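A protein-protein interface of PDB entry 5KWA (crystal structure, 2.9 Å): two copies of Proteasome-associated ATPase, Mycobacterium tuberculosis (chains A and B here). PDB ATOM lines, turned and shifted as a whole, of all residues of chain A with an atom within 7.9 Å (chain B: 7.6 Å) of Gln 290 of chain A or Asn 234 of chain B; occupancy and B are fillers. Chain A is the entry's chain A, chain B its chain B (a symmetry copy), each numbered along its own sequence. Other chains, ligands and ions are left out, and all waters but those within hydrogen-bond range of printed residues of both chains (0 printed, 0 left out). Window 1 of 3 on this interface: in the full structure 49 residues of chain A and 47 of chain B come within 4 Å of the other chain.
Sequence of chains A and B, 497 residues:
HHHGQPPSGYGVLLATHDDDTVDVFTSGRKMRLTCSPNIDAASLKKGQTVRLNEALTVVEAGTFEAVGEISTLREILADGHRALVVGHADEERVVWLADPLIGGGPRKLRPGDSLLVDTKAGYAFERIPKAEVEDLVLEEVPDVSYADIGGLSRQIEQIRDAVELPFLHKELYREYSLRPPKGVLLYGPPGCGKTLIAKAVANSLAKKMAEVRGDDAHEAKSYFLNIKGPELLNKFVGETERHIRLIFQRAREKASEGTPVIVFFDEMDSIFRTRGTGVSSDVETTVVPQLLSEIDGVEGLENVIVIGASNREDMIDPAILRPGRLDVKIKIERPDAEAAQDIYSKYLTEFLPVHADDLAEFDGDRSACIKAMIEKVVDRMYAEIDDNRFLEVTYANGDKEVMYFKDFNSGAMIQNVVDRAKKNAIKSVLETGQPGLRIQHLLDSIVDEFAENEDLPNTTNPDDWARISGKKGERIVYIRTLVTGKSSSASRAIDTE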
ATOM      1  N   GLU A 239      30.127 -14.109 -18.016  1.00  0.00           N
ATOM      2  CA  GLU A 239      29.323 -14.238 -16.781  1.00  0.00           C
ATOM      3  C   GLU A 239      29.304 -15.668 -16.227  1.00  0.00           C
ATOM      4  O   GLU A 239      29.585 -16.618 -16.957  1.00  0.00           O
ATOM      5  CB  GLU A 239      27.877 -13.738 -16.990  1.00  0.00           C
ATOM      6  CG  GLU A 239      27.086 -14.454 -18.094  1.00  0.00           C
ATOM      7  CD  GLU A 239      25.585 -14.560 -17.815  1.00  0.00           C
ATOM      8  OE1 GLU A 239      25.061 -15.701 -17.814  1.00  0.00           O
ATOM      9  OE2 GLU A 239      24.929 -13.512 -17.603  1.00  0.00           O
ATOM     10  N   THR A 240      28.924 -15.804 -14.952  1.00  0.00           N
ATOM     11  CA  THR A 240      29.057 -17.072 -14.193  1.00  0.00           C
ATOM     12  C   THR A 240      28.326 -18.276 -14.789  1.00  0.00           C
ATOM     13  O   THR A 240      28.733 -19.419 -14.574  1.00  0.00           O
ATOM     14  CB  THR A 240      28.560 -16.949 -12.727  1.00  0.00           C
ATOM     15  OG1 THR A 240      27.151 -16.677 -12.707  1.00  0.00           O
ATOM     16  CG2 THR A 240      29.318 -15.866 -11.962  1.00  0.00           C
ATOM     17  N   GLU A 241      27.238 -18.021 -15.504  1.00  0.00           N
ATOM     18  CA  GLU A 241      26.418 -19.091 -16.062  1.00  0.00           C
ATOM     19  C   GLU A 241      26.841 -19.476 -17.490  1.00  0.00           C
ATOM     20  O   GLU A 241      26.470 -20.545 -17.987  1.00  0.00           O
ATOM     21  CB  GLU A 241      24.940 -18.708 -15.957  1.00  0.00           C
ATOM     22  CG  GLU A 241      24.539 -18.252 -14.544  1.00  0.00           C
ATOM     23  CD  GLU A 241      23.122 -18.638 -14.142  1.00  0.00           C
ATOM     24  OE1 GLU A 241      22.173 -18.351 -14.905  1.00  0.00           O
ATOM     25  OE2 GLU A 241      22.958 -19.244 -13.057  1.00  0.00           O
ATOM     26  N   ARG A 242      27.627 -18.614 -18.135  1.00  0.00           N
ATOM     27  CA  ARG A 242      28.327 -18.969 -19.369  1.00  0.00           C
ATOM     28  C   ARG A 242      29.454 -19.965 -19.085  1.00  0.00           C
ATOM     29  O   ARG A 242      29.665 -20.890 -19.868  1.00  0.00           O
ATOM     30  CB  ARG A 242      28.907 -17.724 -20.044  1.00  0.00           C
ATOM     31  CG  ARG A 242      29.335 -17.957 -21.484  1.00  0.00           C
ATOM     32  CD  ARG A 242      30.608 -17.215 -21.850  1.00  0.00           C
ATOM     33  NE  ARG A 242      31.230 -17.827 -23.023  1.00  0.00           N
ATOM     34  CZ  ARG A 242      32.415 -17.491 -23.524  1.00  0.00           C
ATOM     35  NH1 ARG A 242      33.141 -16.521 -22.975  1.00  0.00           N
ATOM     36  NH2 ARG A 242      32.880 -18.133 -24.592  1.00  0.00           N
ATOM     37  N   HIS A 243      30.184 -19.753 -17.983  1.00  0.00           N
ATOM     38  CA  HIS A 243      31.183 -20.719 -17.485  1.00  0.00           C
ATOM     39  C   HIS A 243      30.582 -22.119 -17.371  1.00  0.00           C
ATOM     40  O   HIS A 243      31.159 -23.093 -17.848  1.00  0.00           O
ATOM     41  CB  HIS A 243      31.699 -20.328 -16.093  1.00  0.00           C
ATOM     42  CG  HIS A 243      32.661 -19.181 -16.083  1.00  0.00           C
ATOM     43  ND1 HIS A 243      34.016 -19.351 -15.909  1.00  0.00           N
ATOM     44  CD2 HIS A 243      32.461 -17.848 -16.187  1.00  0.00           C
ATOM     45  CE1 HIS A 243      34.611 -18.173 -15.924  1.00  0.00           C
ATOM     46  NE2 HIS A 243      33.690 -17.243 -16.092  1.00  0.00           N
ATOM     47  N   ILE A 244      29.417 -22.195 -16.732  1.00  0.00           N
ATOM     48  CA  ILE A 244      28.738 -23.464 -16.487  1.00  0.00           C
ATOM     49  C   ILE A 244      28.227 -24.073 -17.798  1.00  0.00           C
ATOM     50  O   ILE A 244      28.297 -25.287 -17.966  1.00  0.00           O
ATOM     51  CB  ILE A 244      27.613 -23.320 -15.425  1.00  0.00           C
ATOM     52  CG1 ILE A 244      28.216 -22.928 -14.067  1.00  0.00           C
ATOM     53  CG2 ILE A 244      26.834 -24.623 -15.255  1.00  0.00           C
ATOM     54  CD1 ILE A 244      27.228 -22.307 -13.103  1.00  0.00           C
ATOM     55  N   ARG A 245      27.739 -23.251 -18.727  1.00  0.00           N
ATOM     56  CA  ARG A 245      27.355 -23.774 -20.040  1.00  0.00           C
ATOM     57  C   ARG A 245      28.556 -24.444 -20.712  1.00  0.00           C
ATOM     58  O   ARG A 245      28.457 -25.594 -21.142  1.00  0.00           O
ATOM     59  CB  ARG A 245      26.758 -22.694 -20.960  1.00  0.00           C
ATOM     60  CG  ARG A 245      26.139 -23.278 -22.244  1.00  0.00           C
ATOM     61  CD  ARG A 245      25.841 -22.242 -23.330  1.00  0.00           C
ATOM     62  NE  ARG A 245      24.406 -22.027 -23.562  1.00  0.00           N
ATOM     63  CZ  ARG A 245      23.900 -21.194 -24.476  1.00  0.00           C
ATOM     64  NH1 ARG A 245      24.696 -20.463 -25.258  1.00  0.00           N
ATOM     65  NH2 ARG A 245      22.579 -21.084 -24.606  1.00  0.00           N
ATOM     66  N   LEU A 246      29.680 -23.729 -20.773  1.00  0.00           N
ATOM     67  CA  LEU A 246      30.913 -24.233 -21.402  1.00  0.00           C
ATOM     68  C   LEU A 246      31.396 -25.557 -20.814  1.00  0.00           C
ATOM     69  O   LEU A 246      31.770 -26.462 -21.561  1.00  0.00           O
ATOM     70  CB  LEU A 246      32.042 -23.202 -21.297  1.00  0.00           C
ATOM     71  CG  LEU A 246      31.894 -21.939 -22.148  1.00  0.00           C
ATOM     72  CD1 LEU A 246      32.821 -20.846 -21.644  1.00  0.00           C
ATOM     73  CD2 LEU A 246      32.155 -22.221 -23.622  1.00  0.00           C
ATOM     74  N   PHE A 248      29.705 -27.948 -18.969  1.00  0.00           N
ATOM     75  CA  PHE A 248      28.761 -29.036 -19.268  1.00  0.00           C
ATOM     76  C   PHE A 248      28.658 -29.356 -20.755  1.00  0.00           C
ATOM     77  O   PHE A 248      28.353 -30.495 -21.111  1.00  0.00           O
ATOM     78  CB  PHE A 248      27.362 -28.728 -18.724  1.00  0.00           C
ATOM     79  CG  PHE A 248      27.190 -29.058 -17.271  1.00  0.00           C
ATOM     80  CD1 PHE A 248      27.301 -28.076 -16.300  1.00  0.00           C
ATOM     81  CD2 PHE A 248      26.905 -30.355 -16.873  1.00  0.00           C
ATOM     82  CE1 PHE A 248      27.131 -28.384 -14.959  1.00  0.00           C
ATOM     83  CE2 PHE A 248      26.735 -30.673 -15.536  1.00  0.00           C
ATOM     84  CZ  PHE A 248      26.847 -29.686 -14.575  1.00  0.00           C
ATOM     85  N   VAL A 287      25.938 -18.710 -10.359  1.00  0.00           N
ATOM     86  CA  VAL A 287      24.821 -18.793  -9.418  1.00  0.00           C
ATOM     87  C   VAL A 287      24.072 -20.124  -9.677  1.00  0.00           C
ATOM     88  O   VAL A 287      24.204 -20.724 -10.755  1.00  0.00           O
ATOM     89  CB  VAL A 287      23.959 -17.474  -9.442  1.00  0.00           C
ATOM     90  CG1 VAL A 287      23.294 -17.230 -10.793  1.00  0.00           C
ATOM     91  CG2 VAL A 287      22.942 -17.414  -8.302  1.00  0.00           C
ATOM     92  N   VAL A 288      23.323 -20.593  -8.676  1.00  0.00           N
ATOM     93  CA  VAL A 288      22.836 -21.985  -8.638  1.00  0.00           C
ATOM     94  C   VAL A 288      21.856 -22.414  -9.744  1.00  0.00           C
ATOM     95  O   VAL A 288      21.892 -23.574 -10.146  1.00  0.00           O
ATOM     96  CB  VAL A 288      22.249 -22.395  -7.243  1.00  0.00           C
ATOM     97  CG1 VAL A 288      23.160 -21.947  -6.109  1.00  0.00           C
ATOM     98  CG2 VAL A 288      20.837 -21.870  -7.006  1.00  0.00           C
ATOM     99  N   PRO A 289      20.976 -21.503 -10.226  1.00  0.00           N
ATOM    100  CA  PRO A 289      19.953 -21.942 -11.172  1.00  0.00           C
ATOM    101  C   PRO A 289      20.472 -22.643 -12.417  1.00  0.00           C
ATOM    102  O   PRO A 289      19.934 -23.692 -12.764  1.00  0.00           O
ATOM    103  CB  PRO A 289      19.253 -20.640 -11.547  1.00  0.00           C
ATOM    104  CG  PRO A 289      19.371 -19.823 -10.318  1.00  0.00           C
ATOM    105  CD  PRO A 289      20.782 -20.081  -9.896  1.00  0.00           C
ATOM    106  N   GLN A 290      21.497 -22.093 -13.073  1.00  0.00           N
ATOM    107  CA  GLN A 290      22.068 -22.763 -14.256  1.00  0.00           C
ATOM    108  C   GLN A 290      22.776 -24.060 -13.911  1.00  0.00           C
ATOM    109  O   GLN A 290      22.819 -24.967 -14.740  1.00  0.00           O
ATOM    110  CB  GLN A 290      22.999 -21.862 -15.081  1.00  0.00           C
ATOM    111  CG  GLN A 290      22.319 -21.248 -16.313  1.00  0.00           C
ATOM    112  CD  GLN A 290      22.429 -22.121 -17.562  1.00  0.00           C
ATOM    113  OE1 GLN A 290      23.525 -22.522 -17.972  1.00  0.00           O
ATOM    114  NE2 GLN A 290      21.287 -22.409 -18.179  1.00  0.00           N
ATOM    115  N   LEU A 291      23.323 -24.155 -12.704  1.00  0.00           N
ATOM    116  CA  LEU A 291      23.904 -25.410 -12.246  1.00  0.00           C
ATOM    117  C   LEU A 291      22.805 -26.467 -12.134  1.00  0.00           C
ATOM    118  O   LEU A 291      22.901 -27.521 -12.763  1.00  0.00           O
ATOM    119  CB  LEU A 291      24.648 -25.221 -10.921  1.00  0.00           C
ATOM    120  CG  LEU A 291      25.483 -26.397 -10.405  1.00  0.00           C
ATOM    121  CD1 LEU A 291      26.457 -26.951 -11.438  1.00  0.00           C
ATOM    122  CD2 LEU A 291      26.234 -25.950  -9.161  1.00  0.00           C
ATOM    123  N   LEU A 292      21.745 -26.151 -11.384  1.00  0.00           N
ATOM    124  CA  LEU A 292      20.574 -27.042 -11.228  1.00  0.00           C
ATOM    125  C   LEU A 292      19.969 -27.455 -12.563  1.00  0.00           C
ATOM    126  O   LEU A 292      19.632 -28.620 -12.769  1.00  0.00           O
ATOM    127  CB  LEU A 292      19.477 -26.377 -10.392  1.00  0.00           C
ATOM    128  CG  LEU A 292      19.780 -26.091  -8.923  1.00  0.00           C
ATOM    129  CD1 LEU A 292      18.631 -25.322  -8.300  1.00  0.00           C
ATOM    130  CD2 LEU A 292      20.038 -27.370  -8.150  1.00  0.00           C
ATOM    131  N   SER A 293      19.840 -26.483 -13.457  1.00  0.00           N
ATOM    132  CA  SER A 293      19.280 -26.712 -14.779  1.00  0.00           C
ATOM    133  C   SER A 293      20.186 -27.619 -15.618  1.00  0.00           C
ATOM    134  O   SER A 293      19.699 -28.554 -16.251  1.00  0.00           O
ATOM    135  CB  SER A 293      19.033 -25.381 -15.488  1.00  0.00           C
ATOM    136  OG  SER A 293      18.076 -25.536 -16.509  1.00  0.00           O
ATOM    137  N   GLU A 294      21.497 -27.364 -15.595  1.00  0.00           N
ATOM    138  CA  GLU A 294      22.468 -28.174 -16.369  1.00  0.00           C
ATOM    139  C   GLU A 294      22.719 -29.584 -15.822  1.00  0.00           C
ATOM    140  O   GLU A 294      23.055 -30.476 -16.594  1.00  0.00           O
ATOM    141  CB  GLU A 294      23.813 -27.444 -16.547  1.00  0.00           C
ATOM    142  CG  GLU A 294      23.836 -26.448 -17.705  1.00  0.00           C
ATOM    143  CD  GLU A 294      23.935 -27.103 -19.085  1.00  0.00           C
ATOM    144  OE1 GLU A 294      23.865 -28.355 -19.200  1.00  0.00           O
ATOM    145  OE2 GLU A 294      24.087 -26.349 -20.074  1.00  0.00           O
ATOM    146  N   ILE A 295      22.588 -29.767 -14.506  1.00  0.00           N
ATOM    147  CA  ILE A 295      22.601 -31.104 -13.898  1.00  0.00           C
ATOM    148  C   ILE A 295      21.342 -31.869 -14.302  1.00  0.00           C
ATOM    149  O   ILE A 295      21.422 -33.046 -14.668  1.00  0.00           O
ATOM    150  CB  ILE A 295      22.702 -31.049 -12.352  1.00  0.00           C
ATOM    151  CG1 ILE A 295      24.080 -30.520 -11.933  1.00  0.00           C
ATOM    152  CG2 ILE A 295      22.475 -32.432 -11.733  1.00  0.00           C
ATOM    153  CD1 ILE A 295      24.177 -30.109 -10.476  1.00  0.00           C
ATOM    154  N   ASP A 296      20.188 -31.207 -14.212  1.00  0.00           N
ATOM    155  CA  ASP A 296      18.917 -31.799 -14.638  1.00  0.00           C
ATOM    156  C   ASP A 296      18.926 -32.162 -16.123  1.00  0.00           C
ATOM    157  O   ASP A 296      18.385 -33.193 -16.492  1.00  0.00           O
ATOM    158  CB  ASP A 296      17.724 -30.866 -14.331  1.00  0.00           C
ATOM    159  CG  ASP A 296      17.268 -30.922 -12.862  1.00  0.00           C
ATOM    160  OD1 ASP A 296      17.781 -31.737 -12.062  1.00  0.00           O
ATOM    161  OD2 ASP A 296      16.367 -30.137 -12.500  1.00  0.00           O
ATOM    162  N   GLY A 297      19.536 -31.317 -16.958  1.00  0.00           N
ATOM    163  CA  GLY A 297      19.653 -31.576 -18.402  1.00  0.00           C
ATOM    164  C   GLY A 297      20.577 -32.728 -18.783  1.00  0.00           C
ATOM    165  O   GLY A 297      20.324 -33.440 -19.756  1.00  0.00           O
ATOM    166  N   GLU B 132      16.472 -24.090 -26.811  1.00  0.00           N
ATOM    167  CA  GLU B 132      16.207 -23.327 -25.569  1.00  0.00           C
ATOM    168  C   GLU B 132      14.843 -22.759 -25.319  1.00  0.00           C
ATOM    169  O   GLU B 132      14.281 -22.979 -24.284  1.00  0.00           O
ATOM    170  CB  GLU B 132      17.260 -22.285 -25.226  1.00  0.00           C
ATOM    171  CG  GLU B 132      18.660 -22.816 -25.330  1.00  0.00           C
ATOM    172  CD  GLU B 132      19.176 -23.358 -24.032  1.00  0.00           C
ATOM    173  OE1 GLU B 132      18.792 -24.476 -23.648  1.00  0.00           O
ATOM    174  OE2 GLU B 132      19.982 -22.659 -23.405  1.00  0.00           O
ATOM    175  N   LEU B 136      12.140 -25.133 -23.586  1.00  0.00           N
ATOM    176  CA  LEU B 136      11.476 -24.538 -22.414  1.00  0.00           C
ATOM    177  C   LEU B 136       9.975 -24.792 -22.454  1.00  0.00           C
ATOM    178  O   LEU B 136       9.391 -25.289 -21.491  1.00  0.00           O
ATOM    179  CB  LEU B 136      11.720 -23.027 -22.359  1.00  0.00           C
ATOM    180  CG  LEU B 136      10.918 -22.212 -21.351  1.00  0.00           C
ATOM    181  CD1 LEU B 136      11.134 -22.742 -19.943  1.00  0.00           C
ATOM    182  CD2 LEU B 136      11.315 -20.749 -21.453  1.00  0.00           C
ATOM    183  N   GLY B 229      11.220 -24.329 -11.705  1.00  0.00           N
ATOM    184  CA  GLY B 229      11.608 -22.977 -11.268  1.00  0.00           C
ATOM    185  C   GLY B 229      12.913 -22.423 -11.832  1.00  0.00           C
ATOM    186  O   GLY B 229      12.913 -21.355 -12.452  1.00  0.00           O
ATOM    187  N   PRO B 230      14.027 -23.144 -11.618  1.00  0.00           N
ATOM    188  CA  PRO B 230      15.333 -22.827 -12.202  1.00  0.00           C
ATOM    189  C   PRO B 230      15.345 -22.511 -13.712  1.00  0.00           C
ATOM    190  O   PRO B 230      16.087 -21.618 -14.133  1.00  0.00           O
ATOM    191  CB  PRO B 230      16.136 -24.095 -11.923  1.00  0.00           C
ATOM    192  CG  PRO B 230      15.589 -24.578 -10.624  1.00  0.00           C
ATOM    193  CD  PRO B 230      14.130 -24.239 -10.633  1.00  0.00           C
ATOM    194  N   GLU B 231      14.535 -23.222 -14.504  1.00  0.00           N
ATOM    195  CA  GLU B 231      14.437 -22.976 -15.957  1.00  0.00           C
ATOM    196  C   GLU B 231      14.042 -21.537 -16.308  1.00  0.00           C
ATOM    197  O   GLU B 231      14.388 -21.062 -17.382  1.00  0.00           O
ATOM    198  CB  GLU B 231      13.438 -23.930 -16.642  1.00  0.00           C
ATOM    199  CG  GLU B 231      13.820 -25.405 -16.657  1.00  0.00           C
ATOM    200  CD  GLU B 231      12.814 -26.274 -17.410  1.00  0.00           C
ATOM    201  OE1 GLU B 231      12.466 -27.365 -16.912  1.00  0.00           O
ATOM    202  OE2 GLU B 231      12.356 -25.877 -18.501  1.00  0.00           O
ATOM    203  N   LEU B 232      13.309 -20.860 -15.423  1.00  0.00           N
ATOM    204  CA  LEU B 232      12.887 -19.473 -15.649  1.00  0.00           C
ATOM    205  C   LEU B 232      14.031 -18.473 -15.494  1.00  0.00           C
ATOM    206  O   LEU B 232      14.107 -17.495 -16.241  1.00  0.00           O
ATOM    207  CB  LEU B 232      11.756 -19.089 -14.687  1.00  0.00           C
ATOM    208  CG  LEU B 232      10.471 -19.920 -14.729  1.00  0.00           C
ATOM    209  CD1 LEU B 232       9.482 -19.413 -13.686  1.00  0.00           C
ATOM    210  CD2 LEU B 232       9.859 -19.893 -16.122  1.00  0.00           C
ATOM    211  N   LEU B 233      14.915 -18.727 -14.529  1.00  0.00           N
ATOM    212  CA  LEU B 233      16.013 -17.808 -14.207  1.00  0.00           C
ATOM    213  C   LEU B 233      17.174 -17.844 -15.210  1.00  0.00           C
ATOM    214  O   LEU B 233      17.992 -16.925 -15.220  1.00  0.00           O
ATOM    215  CB  LEU B 233      16.529 -18.071 -12.786  1.00  0.00           C
ATOM    216  CG  LEU B 233      15.474 -18.087 -11.665  1.00  0.00           C
ATOM    217  CD1 LEU B 233      16.131 -18.247 -10.300  1.00  0.00           C
ATOM    218  CD2 LEU B 233      14.597 -16.844 -11.691  1.00  0.00           C
ATOM    219  N   ASN B 234      17.244 -18.892 -16.037  1.00  0.00           N
ATOM    220  CA  ASN B 234      18.231 -19.012 -17.134  1.00  0.00           C
ATOM    221  C   ASN B 234      18.585 -17.658 -17.801  1.00  0.00           C
ATOM    222  O   ASN B 234      18.220 -17.373 -18.941  1.00  0.00           O
ATOM    223  CB  ASN B 234      17.722 -20.044 -18.168  1.00  0.00           C
ATOM    224  CG  ASN B 234      18.768 -20.432 -19.207  1.00  0.00           C
ATOM    225  OD1 ASN B 234      19.743 -19.715 -19.450  1.00  0.00           O
ATOM    226  ND2 ASN B 234      18.558 -21.580 -19.838  1.00  0.00           N
ATOM    227  N   GLY B 238      16.269 -15.260 -22.653  1.00  0.00           N
ATOM    228  CA  GLY B 238      16.370 -13.899 -22.117  1.00  0.00           C
ATOM    229  C   GLY B 238      16.079 -13.778 -20.623  1.00  0.00           C
ATOM    230  O   GLY B 238      16.424 -14.666 -19.850  1.00  0.00           O
ATOM    231  N   GLU B 239      15.447 -12.670 -20.223  1.00  0.00           N
ATOM    232  CA  GLU B 239      15.123 -12.387 -18.810  1.00  0.00           C
ATOM    233  C   GLU B 239      13.734 -12.958 -18.469  1.00  0.00           C
ATOM    234  O   GLU B 239      12.895 -13.086 -19.360  1.00  0.00           O
ATOM    235  CB  GLU B 239      15.190 -10.868 -18.550  1.00  0.00           C
ATOM    236  CG  GLU B 239      15.793 -10.454 -17.202  1.00  0.00           C
ATOM    237  CD  GLU B 239      14.818 -10.493 -16.026  1.00  0.00           C
ATOM    238  OE1 GLU B 239      13.610 -10.758 -16.216  1.00  0.00           O
ATOM    239  OE2 GLU B 239      15.267 -10.248 -14.887  1.00  0.00           O
ATOM    240  N   THR B 240      13.506 -13.292 -17.189  1.00  0.00           N
ATOM    241  CA  THR B 240      12.271 -13.987 -16.713  1.00  0.00           C
ATOM    242  C   THR B 240      10.935 -13.525 -17.323  1.00  0.00           C
ATOM    243  O   THR B 240      10.019 -14.328 -17.476  1.00  0.00           O
ATOM    244  CB  THR B 240      12.107 -13.925 -15.168  1.00  0.00           C
ATOM    245  OG1 THR B 240      12.025 -12.561 -14.739  1.00  0.00           O
ATOM    246  CG2 THR B 240      13.253 -14.624 -14.442  1.00  0.00           C
ATOM    247  N   HIS B 243      10.563 -15.394 -20.510  1.00  0.00           N
ATOM    248  CA  HIS B 243      10.283 -16.811 -20.203  1.00  0.00           C
ATOM    249  C   HIS B 243       8.797 -17.045 -20.011  1.00  0.00           C
ATOM    250  O   HIS B 243       8.220 -17.926 -20.643  1.00  0.00           O
ATOM    251  CB  HIS B 243      11.004 -17.272 -18.933  1.00  0.00           C
ATOM    252  CG  HIS B 243      12.474 -17.488 -19.106  1.00  0.00           C
ATOM    253  ND1 HIS B 243      13.034 -18.742 -19.207  1.00  0.00           N
ATOM    254  CD2 HIS B 243      13.504 -16.611 -19.174  1.00  0.00           C
ATOM    255  CE1 HIS B 243      14.343 -18.630 -19.339  1.00  0.00           C
ATOM    256  NE2 HIS B 243      14.655 -17.348 -19.318  1.00  0.00           N
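NH2 of Arg 245 of chain A lies within salt-bridge range of OE2 of Glu 132 of chain B (3.3 Å).
NE2 of Gln 290 of chain A sits close to ND2 of Asn 234 of chain B (3.3 Å).
OE2 of Glu 241 of chain A lies within hydrogen-bond range of N of Gln 290 of chain A, 3.2 Å away.
Among the printed residues, merely in contact across the chains: Pro 289 of chain A with Leu 233 of chain B, Leu 292 of chain A with Pro 230 of chain B and Pro 289 of chain A with Pro 230 of chain B.
Printed residues of chain B within 4 Å of Arg 245 of chain A: Glu 132.
Printed residues of chain B within 4 Å of Gln 290 of chain A: Asn 234.
Asp 296 of chain A touches none of the printed residues of chain B.
Printed residues of chain A within 4 Å of Pro 230 of chain B: Pro 289 (3.9 Å) and Leu 292 (3.9 Å).
Of the printed residues of chain A, Leu 233 of chain B touches Pro 289 (3.6 Å).
Of the printed residues of chain A, Asn 234 of chain B touches Gln 290.
Gly 238 of chain B touches none of the printed residues of chain A.
The nearest residue of chain B that does not touch Gln 290 of chain A is Glu 132 of chain B (5.4 Å).
The nearest residue of chain A that does not touch Asn 234 of chain B is Glu 241 of chain A (4.6 Å).
The nearest printed residue of chain B that does not touch Leu 292 of chain A is Glu 231 of chain B (7.2 Å).
Of the 12 printed residues of chain B, 4 touch a printed residue of chain A.
Hydrophobic or aromatic side chains of chain B within 4 Å of the printed part of chain A: Pro 230 and Leu 233.
Of the 20 printed residues of chain A, 4 touch a printed residue of chain B.
Printed residues of chain A that touch a printed residue of chain B: Arg 245, Pro 289, Gln 290 and Leu 292.
Hydrophobic or aromatic side chains of chain A within 4 Å of the printed part of chain B: Pro 289 and Leu 292.
Among the printed residues, 5 pairs touch across the chains.
3 positions are printed for both chains.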
